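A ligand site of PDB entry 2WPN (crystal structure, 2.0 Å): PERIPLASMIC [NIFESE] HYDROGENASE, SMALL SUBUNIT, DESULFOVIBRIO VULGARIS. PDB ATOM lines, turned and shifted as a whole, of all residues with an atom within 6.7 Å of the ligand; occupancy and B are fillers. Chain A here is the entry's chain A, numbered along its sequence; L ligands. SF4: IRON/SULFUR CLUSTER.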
ATOM      1  N   ASN A 240     -18.299 -10.473 -23.377  1.00  0.00           N
ATOM      2  CA  ASN A 240     -19.145 -10.030 -22.268  1.00  0.00           C
ATOM      3  C   ASN A 240     -20.589  -9.785 -22.744  1.00  0.00           C
ATOM      4  O   ASN A 240     -20.775  -9.129 -23.748  1.00  0.00           O
ATOM      5  CB  ASN A 240     -18.547  -8.739 -21.710  1.00  0.00           C
ATOM      6  CG  ASN A 240     -19.397  -8.132 -20.624  1.00  0.00           C
ATOM      7  OD1 ASN A 240     -20.119  -7.184 -20.878  1.00  0.00           O
ATOM      8  ND2 ASN A 240     -19.327  -8.698 -19.419  1.00  0.00           N
ATOM      9  N   ILE A 241     -21.600 -10.320 -22.037  1.00  0.00           N
ATOM     10  CA  ILE A 241     -23.003 -10.150 -22.473  1.00  0.00           C
ATOM     11  C   ILE A 241     -23.407  -8.666 -22.606  1.00  0.00           C
ATOM     12  O   ILE A 241     -23.981  -8.247 -23.626  1.00  0.00           O
ATOM     13  CB  ILE A 241     -23.994 -10.891 -21.528  1.00  0.00           C
ATOM     14  CG1 ILE A 241     -23.755 -12.402 -21.632  1.00  0.00           C
ATOM     15  CG2 ILE A 241     -25.452 -10.440 -21.821  1.00  0.00           C
ATOM     16  CD1 ILE A 241     -24.701 -13.291 -20.878  1.00  0.00           C
ATOM     17  N   HIS A 242     -23.098  -7.903 -21.559  1.00  0.00           N
ATOM     18  CA  HIS A 242     -23.515  -6.501 -21.412  1.00  0.00           C
ATOM     19  C   HIS A 242     -22.934  -5.601 -22.501  1.00  0.00           C
ATOM     20  O   HIS A 242     -23.664  -4.786 -23.080  1.00  0.00           O
ATOM     21  CB  HIS A 242     -23.141  -6.017 -20.012  1.00  0.00           C
ATOM     22  CG  HIS A 242     -23.389  -4.553 -19.754  1.00  0.00           C
ATOM     23  ND1 HIS A 242     -24.639  -4.040 -19.493  1.00  0.00           N
ATOM     24  CD2 HIS A 242     -22.519  -3.514 -19.681  1.00  0.00           C
ATOM     25  CE1 HIS A 242     -24.524  -2.735 -19.273  1.00  0.00           C
ATOM     26  NE2 HIS A 242     -23.253  -2.390 -19.382  1.00  0.00           N
ATOM     27  N   GLU A 243     -21.636  -5.749 -22.786  1.00  0.00           N
ATOM     28  CA  GLU A 243     -20.973  -4.982 -23.878  1.00  0.00           C
ATOM     29  C   GLU A 243     -21.596  -5.275 -25.241  1.00  0.00           C
ATOM     30  O   GLU A 243     -21.479  -4.480 -26.160  1.00  0.00           O
ATOM     31  CB  GLU A 243     -19.489  -5.310 -23.925  1.00  0.00           C
ATOM     32  CG  GLU A 243     -18.649  -4.695 -22.802  1.00  0.00           C
ATOM     33  CD  GLU A 243     -17.257  -5.320 -22.749  1.00  0.00           C
ATOM     34  OE1 GLU A 243     -16.876  -6.005 -23.717  1.00  0.00           O
ATOM     35  OE2 GLU A 243     -16.544  -5.144 -21.734  1.00  0.00           O
ATOM     36  N   CYS A 245     -24.992  -6.304 -25.468  1.00  0.00           N
ATOM     37  CA  CYS A 245     -26.412  -6.416 -25.200  1.00  0.00           C
ATOM     38  C   CYS A 245     -27.232  -5.405 -26.042  1.00  0.00           C
ATOM     39  O   CYS A 245     -26.832  -4.226 -26.192  1.00  0.00           O
ATOM     40  CB  CYS A 245     -26.700  -6.252 -23.703  1.00  0.00           C
ATOM     41  SG  CYS A 245     -28.451  -6.457 -23.283  1.00  0.00           S
ATOM     42  N   PRO A 246     -28.372  -5.849 -26.604  1.00  0.00           N
ATOM     43  CA  PRO A 246     -29.189  -4.900 -27.364  1.00  0.00           C
ATOM     44  C   PRO A 246     -29.792  -3.766 -26.529  1.00  0.00           C
ATOM     45  O   PRO A 246     -30.194  -2.780 -27.109  1.00  0.00           O
ATOM     46  CB  PRO A 246     -30.315  -5.764 -27.988  1.00  0.00           C
ATOM     47  CG  PRO A 246     -30.156  -7.103 -27.474  1.00  0.00           C
ATOM     48  CD  PRO A 246     -28.885  -7.235 -26.677  1.00  0.00           C
ATOM     49  N   TYR A 247     -29.818  -3.895 -25.205  1.00  0.00           N
ATOM     50  CA  TYR A 247     -30.331  -2.846 -24.319  1.00  0.00           C
ATOM     51  C   TYR A 247     -29.234  -1.956 -23.750  1.00  0.00           C
ATOM     52  O   TYR A 247     -29.485  -1.140 -22.868  1.00  0.00           O
ATOM     53  CB  TYR A 247     -31.225  -3.428 -23.211  1.00  0.00           C
ATOM     54  CG  TYR A 247     -32.201  -4.445 -23.768  1.00  0.00           C
ATOM     55  CD1 TYR A 247     -33.243  -4.032 -24.631  1.00  0.00           C
ATOM     56  CD2 TYR A 247     -32.063  -5.819 -23.501  1.00  0.00           C
ATOM     57  CE1 TYR A 247     -34.123  -4.976 -25.199  1.00  0.00           C
ATOM     58  CE2 TYR A 247     -32.926  -6.748 -24.047  1.00  0.00           C
ATOM     59  CZ  TYR A 247     -33.961  -6.333 -24.904  1.00  0.00           C
ATOM     60  OH  TYR A 247     -34.823  -7.274 -25.416  1.00  0.00           O
ATOM     61  N   LEU A 248     -28.019  -2.080 -24.279  1.00  0.00           N
ATOM     62  CA  LEU A 248     -26.869  -1.298 -23.797  1.00  0.00           C
ATOM     63  C   LEU A 248     -27.169   0.219 -23.812  1.00  0.00           C
ATOM     64  O   LEU A 248     -26.907   0.916 -22.829  1.00  0.00           O
ATOM     65  CB  LEU A 248     -25.596  -1.662 -24.548  1.00  0.00           C
ATOM     66  CG  LEU A 248     -24.327  -0.953 -24.071  1.00  0.00           C
ATOM     67  CD1 LEU A 248     -24.036  -1.269 -22.613  1.00  0.00           C
ATOM     68  CD2 LEU A 248     -23.118  -1.307 -24.925  1.00  0.00           C
ATOM     69  N   ASP A 249     -27.746   0.701 -24.914  1.00  0.00           N
ATOM     70  CA  ASP A 249     -28.208   2.102 -25.047  1.00  0.00           C
ATOM     71  C   ASP A 249     -29.116   2.529 -23.892  1.00  0.00           C
ATOM     72  O   ASP A 249     -28.965   3.622 -23.358  1.00  0.00           O
ATOM     73  CB  ASP A 249     -28.959   2.289 -26.363  1.00  0.00           C
ATOM     74  CG  ASP A 249     -30.309   1.506 -26.388  1.00  0.00           C
ATOM     75  OD1 ASP A 249     -30.323   0.289 -26.061  1.00  0.00           O
ATOM     76  OD2 ASP A 249     -31.347   2.119 -26.741  1.00  0.00           O
ATOM     77  N   LYS A 250     -30.058   1.673 -23.502  1.00  0.00           N
ATOM     78  CA  LYS A 250     -30.978   2.005 -22.411  1.00  0.00           C
ATOM     79  C   LYS A 250     -30.215   2.093 -21.094  1.00  0.00           C
ATOM     80  O   LYS A 250     -30.434   3.022 -20.304  1.00  0.00           O
ATOM     81  CB  LYS A 250     -32.139   1.015 -22.286  1.00  0.00           C
ATOM     82  CG  LYS A 250     -33.012   0.840 -23.540  1.00  0.00           C
ATOM     83  CD  LYS A 250     -33.769   2.113 -23.914  1.00  0.00           C
ATOM     84  CE  LYS A 250     -34.500   1.932 -25.221  1.00  0.00           C
ATOM     85  NZ  LYS A 250     -34.950   3.227 -25.758  1.00  0.00           N
ATOM     86  N   TYR A 251     -29.313   1.121 -20.883  1.00  0.00           N
ATOM     87  CA  TYR A 251     -28.412   1.143 -19.735  1.00  0.00           C
ATOM     88  C   TYR A 251     -27.645   2.479 -19.677  1.00  0.00           C
ATOM     89  O   TYR A 251     -27.630   3.140 -18.627  1.00  0.00           O
ATOM     90  CB  TYR A 251     -27.441  -0.048 -19.751  1.00  0.00           C
ATOM     91  CG  TYR A 251     -26.445  -0.057 -18.594  1.00  0.00           C
ATOM     92  CD1 TYR A 251     -26.758  -0.649 -17.374  1.00  0.00           C
ATOM     93  CD2 TYR A 251     -25.208   0.568 -18.729  1.00  0.00           C
ATOM     94  CE1 TYR A 251     -25.855  -0.654 -16.315  1.00  0.00           C
ATOM     95  CE2 TYR A 251     -24.274   0.580 -17.665  1.00  0.00           C
ATOM     96  CZ  TYR A 251     -24.607  -0.037 -16.476  1.00  0.00           C
ATOM     97  OH  TYR A 251     -23.704  -0.029 -15.422  1.00  0.00           O
ATOM     98  N   ASP A 252     -27.024   2.885 -20.782  1.00  0.00           N
ATOM     99  CA  ASP A 252     -26.283   4.157 -20.828  1.00  0.00           C
ATOM    100  C   ASP A 252     -27.184   5.391 -20.640  1.00  0.00           C
ATOM    101  O   ASP A 252     -26.747   6.389 -20.077  1.00  0.00           O
ATOM    102  CB  ASP A 252     -25.400   4.285 -22.081  1.00  0.00           C
ATOM    103  CG  ASP A 252     -24.255   3.283 -22.098  1.00  0.00           C
ATOM    104  OD1 ASP A 252     -23.715   2.953 -21.007  1.00  0.00           O
ATOM    105  OD2 ASP A 252     -23.900   2.800 -23.201  1.00  0.00           O
ATOM    106  N   MET A 256     -34.483   2.143 -17.020  1.00  0.00           N
ATOM    107  CA  MET A 256     -34.523   0.841 -16.396  1.00  0.00           C
ATOM    108  C   MET A 256     -35.959   0.420 -16.350  1.00  0.00           C
ATOM    109  O   MET A 256     -36.810   1.216 -15.976  1.00  0.00           O
ATOM    110  CB  MET A 256     -34.019   0.970 -14.978  1.00  0.00           C
ATOM    111  CG  MET A 256     -32.633   1.509 -14.926  1.00  0.00           C
ATOM    112  SD  MET A 256     -31.516   0.252 -15.580  1.00  0.00           S
ATOM    113  CE  MET A 256     -29.938   1.134 -15.588  1.00  0.00           C
ATOM    114  N   GLY A 265     -36.907  -1.172 -21.544  1.00  0.00           N
ATOM    115  CA  GLY A 265     -35.757  -0.695 -20.783  1.00  0.00           C
ATOM    116  C   GLY A 265     -34.717  -1.754 -20.436  1.00  0.00           C
ATOM    117  O   GLY A 265     -34.918  -2.959 -20.637  1.00  0.00           O
ATOM    118  N   CYS A 266     -33.592  -1.288 -19.895  1.00  0.00           N
ATOM    119  CA  CYS A 266     -32.581  -2.173 -19.368  1.00  0.00           C
ATOM    120  C   CYS A 266     -33.054  -2.949 -18.134  1.00  0.00           C
ATOM    121  O   CYS A 266     -33.851  -2.442 -17.296  1.00  0.00           O
ATOM    122  CB  CYS A 266     -31.337  -1.345 -19.029  1.00  0.00           C
ATOM    123  SG  CYS A 266     -30.105  -2.253 -18.059  1.00  0.00           S
ATOM    124  N   ARG A 267     -32.547  -4.184 -18.017  1.00  0.00           N
ATOM    125  CA  ARG A 267     -32.903  -5.114 -16.946  1.00  0.00           C
ATOM    126  C   ARG A 267     -32.011  -4.985 -15.699  1.00  0.00           C
ATOM    127  O   ARG A 267     -32.173  -5.712 -14.704  1.00  0.00           O
ATOM    128  CB  ARG A 267     -32.891  -6.550 -17.473  1.00  0.00           C
ATOM    129  CG  ARG A 267     -34.111  -6.939 -18.325  1.00  0.00           C
ATOM    130  CD  ARG A 267     -34.164  -6.241 -19.674  1.00  0.00           C
ATOM    131  NE  ARG A 267     -34.849  -7.078 -20.666  1.00  0.00           N
ATOM    132  CZ  ARG A 267     -35.553  -6.585 -21.701  1.00  0.00           C
ATOM    133  NH1 ARG A 267     -35.670  -5.289 -21.886  1.00  0.00           N
ATOM    134  NH2 ARG A 267     -36.150  -7.415 -22.562  1.00  0.00           N
ATOM    135  N   TYR A 268     -31.082  -4.041 -15.741  1.00  0.00           N
ATOM    136  CA  TYR A 268     -30.133  -3.926 -14.635  1.00  0.00           C
ATOM    137  C   TYR A 268     -30.810  -3.822 -13.276  1.00  0.00           C
ATOM    138  O   TYR A 268     -30.487  -4.577 -12.383  1.00  0.00           O
ATOM    139  CB  TYR A 268     -29.169  -2.764 -14.856  1.00  0.00           C
ATOM    140  CG  TYR A 268     -28.165  -2.604 -13.752  1.00  0.00           C
ATOM    141  CD1 TYR A 268     -26.963  -3.320 -13.761  1.00  0.00           C
ATOM    142  CD2 TYR A 268     -28.407  -1.741 -12.676  1.00  0.00           C
ATOM    143  CE1 TYR A 268     -26.026  -3.152 -12.721  1.00  0.00           C
ATOM    144  CE2 TYR A 268     -27.514  -1.584 -11.645  1.00  0.00           C
ATOM    145  CZ  TYR A 268     -26.323  -2.286 -11.678  1.00  0.00           C
ATOM    146  OH  TYR A 268     -25.425  -2.109 -10.628  1.00  0.00           O
ATOM    147  N   ASP A 269     -31.768  -2.904 -13.118  1.00  0.00           N
ATOM    148  CA  ASP A 269     -32.448  -2.737 -11.841  1.00  0.00           C
ATOM    149  C   ASP A 269     -33.256  -3.992 -11.406  1.00  0.00           C
ATOM    150  O   ASP A 269     -33.442  -4.242 -10.217  1.00  0.00           O
ATOM    151  CB  ASP A 269     -33.346  -1.495 -11.881  1.00  0.00           C
ATOM    152  CG  ASP A 269     -32.599  -0.203 -11.561  1.00  0.00           C
ATOM    153  OD1 ASP A 269     -31.373  -0.207 -11.340  1.00  0.00           O
ATOM    154  OD2 ASP A 269     -33.274   0.837 -11.509  1.00  0.00           O
ATOM    155  N   CYS A 272     -30.243  -7.923 -13.518  1.00  0.00           N
ATOM    156  CA  CYS A 272     -29.417  -8.440 -14.623  1.00  0.00           C
ATOM    157  C   CYS A 272     -27.939  -8.502 -14.298  1.00  0.00           C
ATOM    158  O   CYS A 272     -27.330  -7.479 -13.929  1.00  0.00           O
ATOM    159  CB  CYS A 272     -29.579  -7.583 -15.883  1.00  0.00           C
ATOM    160  SG  CYS A 272     -28.877  -8.422 -17.317  1.00  0.00           S
ATOM    161  N   LYS A 273     -27.364  -9.680 -14.501  1.00  0.00           N
ATOM    162  CA  LYS A 273     -25.959  -9.909 -14.206  1.00  0.00           C
ATOM    163  C   LYS A 273     -25.078  -9.875 -15.473  1.00  0.00           C
ATOM    164  O   LYS A 273     -23.875 -10.167 -15.408  1.00  0.00           O
ATOM    165  CB  LYS A 273     -25.769 -11.199 -13.398  1.00  0.00           C
ATOM    166  CG  LYS A 273     -26.357 -11.175 -11.973  1.00  0.00           C
ATOM    167  CD  LYS A 273     -26.162  -9.831 -11.214  1.00  0.00           C
ATOM    168  CE  LYS A 273     -26.895  -9.823  -9.851  1.00  0.00           C
ATOM    169  NZ  LYS A 273     -28.314 -10.317  -9.848  1.00  0.00           N
ATOM    170  N   GLY A 274     -25.679  -9.493 -16.606  1.00  0.00           N
ATOM    171  CA  GLY A 274     -24.968  -9.249 -17.856  1.00  0.00           C
ATOM    172  C   GLY A 274     -23.621  -8.517 -17.731  1.00  0.00           C
ATOM    173  O   GLY A 274     -22.645  -8.940 -18.366  1.00  0.00           O
ATOM    174  N   PRO A 275     -23.557  -7.413 -16.924  1.00  0.00           N
ATOM    175  CA  PRO A 275     -22.277  -6.717 -16.771  1.00  0.00           C
ATOM    176  C   PRO A 275     -21.099  -7.585 -16.320  1.00  0.00           C
ATOM    177  O   PRO A 275     -19.961  -7.269 -16.674  1.00  0.00           O
ATOM    178  CB  PRO A 275     -22.584  -5.631 -15.712  1.00  0.00           C
ATOM    179  CG  PRO A 275     -24.016  -5.260 -15.977  1.00  0.00           C
ATOM    180  CD  PRO A 275     -24.651  -6.660 -16.249  1.00  0.00           C
ATOM    181  N   TRP A 292     -33.948 -15.757 -25.086  1.00  0.00           N
ATOM    182  CA  TRP A 292     -32.786 -15.850 -24.205  1.00  0.00           C
ATOM    183  C   TRP A 292     -33.036 -15.106 -22.874  1.00  0.00           C
ATOM    184  O   TRP A 292     -34.003 -14.326 -22.752  1.00  0.00           O
ATOM    185  CB  TRP A 292     -31.513 -15.392 -24.941  1.00  0.00           C
ATOM    186  CG  TRP A 292     -31.411 -13.948 -25.212  1.00  0.00           C
ATOM    187  CD1 TRP A 292     -32.245 -13.188 -25.982  1.00  0.00           C
ATOM    188  CD2 TRP A 292     -30.392 -13.063 -24.724  1.00  0.00           C
ATOM    189  NE1 TRP A 292     -31.823 -11.879 -25.982  1.00  0.00           N
ATOM    190  CE2 TRP A 292     -30.675 -11.776 -25.232  1.00  0.00           C
ATOM    191  CE3 TRP A 292     -29.252 -13.234 -23.901  1.00  0.00           C
ATOM    192  CZ2 TRP A 292     -29.883 -10.668 -24.933  1.00  0.00           C
ATOM    193  CZ3 TRP A 292     -28.450 -12.115 -23.617  1.00  0.00           C
ATOM    194  CH2 TRP A 292     -28.773 -10.861 -24.131  1.00  0.00           C
ATOM    195  N   VAL A 294     -31.957 -12.629 -21.142  1.00  0.00           N
ATOM    196  CA  VAL A 294     -32.099 -11.177 -21.020  1.00  0.00           C
ATOM    197  C   VAL A 294     -33.380 -10.637 -21.678  1.00  0.00           C
ATOM    198  O   VAL A 294     -34.045  -9.757 -21.124  1.00  0.00           O
ATOM    199  CB  VAL A 294     -30.825 -10.406 -21.470  1.00  0.00           C
ATOM    200  CG1 VAL A 294     -31.073  -8.916 -21.458  1.00  0.00           C
ATOM    201  CG2 VAL A 294     -29.635 -10.759 -20.595  1.00  0.00           C
ATOM    202  N   ALA A 297     -36.291 -12.296 -19.159  1.00  0.00           N
ATOM    203  CA  ALA A 297     -36.274 -11.921 -17.745  1.00  0.00           C
ATOM    204  C   ALA A 297     -34.952 -11.188 -17.385  1.00  0.00           C
ATOM    205  O   ALA A 297     -34.820 -10.023 -17.674  1.00  0.00           O
ATOM    206  CB  ALA A 297     -36.524 -13.185 -16.824  1.00  0.00           C
ATOM    207  N   CYS A 299     -30.355 -11.958 -16.887  1.00  0.00           N
ATOM    208  CA  CYS A 299     -29.204 -12.881 -16.843  1.00  0.00           C
ATOM    209  C   CYS A 299     -28.856 -13.115 -15.386  1.00  0.00           C
ATOM    210  O   CYS A 299     -28.845 -12.168 -14.603  1.00  0.00           O
ATOM    211  CB  CYS A 299     -27.976 -12.296 -17.570  1.00  0.00           C
ATOM    212  SG  CYS A 299     -26.483 -13.323 -17.481  1.00  0.00           S
HETATM  213 FE1  SF4 L   1     -28.388  -6.577 -18.624  1.00  0.00          FE
HETATM  214 FE2  SF4 L   1     -29.013  -3.964 -19.158  1.00  0.00          FE
HETATM  215 FE3  SF4 L   1     -28.294  -5.646 -21.142  1.00  0.00          FE
HETATM  216 FE4  SF4 L   1     -26.453  -4.832 -19.444  1.00  0.00          FE
HETATM  217  S1  SF4 L   1     -27.607  -3.490 -20.925  1.00  0.00           S
HETATM  218  S2  SF4 L   1     -26.721  -7.006 -20.146  1.00  0.00           S
HETATM  219  S3  SF4 L   1     -27.648  -4.735 -17.460  1.00  0.00           S
HETATM  220  S4  SF4 L   1     -30.206  -5.803 -19.856  1.00  0.00           S
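The backbone carbonyl oxygen (O) of Tyr 247 lies close to a sulfur (S1) of the ligand.
Tyr 251 touches the ligand (CB to S1, 3.6 Å).
Tyr 268 touches the ligand.
CA of Gly 274 touches S2 of the ligand, at 3.7 Å.
CD of Pro 275 touches S3 of the ligand, at 3.8 Å.
Val 294 touches the ligand (CG1 to S4, 3.6 Å).
Within 4 Å of the ligand: His 242, Cys 245, Tyr 247, Leu 248, Tyr 251, Cys 266, Arg 267, Tyr 268, Cys 272, Gly 274, Pro 275 and Val 294.
An iron atom (FE4) of the ligand is bound by a ring nitrogen (ND1) of His 242 (2.0 Å).
An iron atom (FE3) of the ligand is bound by the side-chain sulfur (SG) of Cys 245, at 2.3 Å.
FE2 of the ligand is bound by SG of Cys 266 (2.3 Å).
An iron atom (FE1) of the ligand is bound by the side-chain sulfur (SG) of Cys 272, 2.3 Å away.
The backbone NH (N) of Arg 267 lies close to a sulfur (S4) of the ligand, at 3.4 Å.
S1 of the ligand sits close to N of Leu 248.
N of His 242 lies within hydrogen-bond range of OD1 of Asn 240.
SD of Met 256 lies close to SG of Cys 266 (3.8 Å).
The backbone NH of Cys 272 sits at hydrogen-bond distance from the backbone carbonyl oxygen of Arg 267 (3.2 Å).
The side-chain sulfur (SG) of Cys 272 lies close to the backbone NH (N) of Gly 274, at 3.4 Å.
OH of Tyr 247 sits at hydrogen-bond distance from NH2 of Arg 267, at 3.2 Å.
NE of Arg 267 sits at hydrogen-bond distance from O of Val 294, at 2.8 Å.
The side-chain amide nitrogen (ND2) of Asn 240 sits at hydrogen-bond distance from the backbone carbonyl oxygen (O) of Gly 274 (3.5 Å).
The backbone carbonyl oxygen (O) of Pro 275 sits at hydrogen-bond distance from the side-chain amide nitrogen (ND2) of Asn 240, at 3.2 Å.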
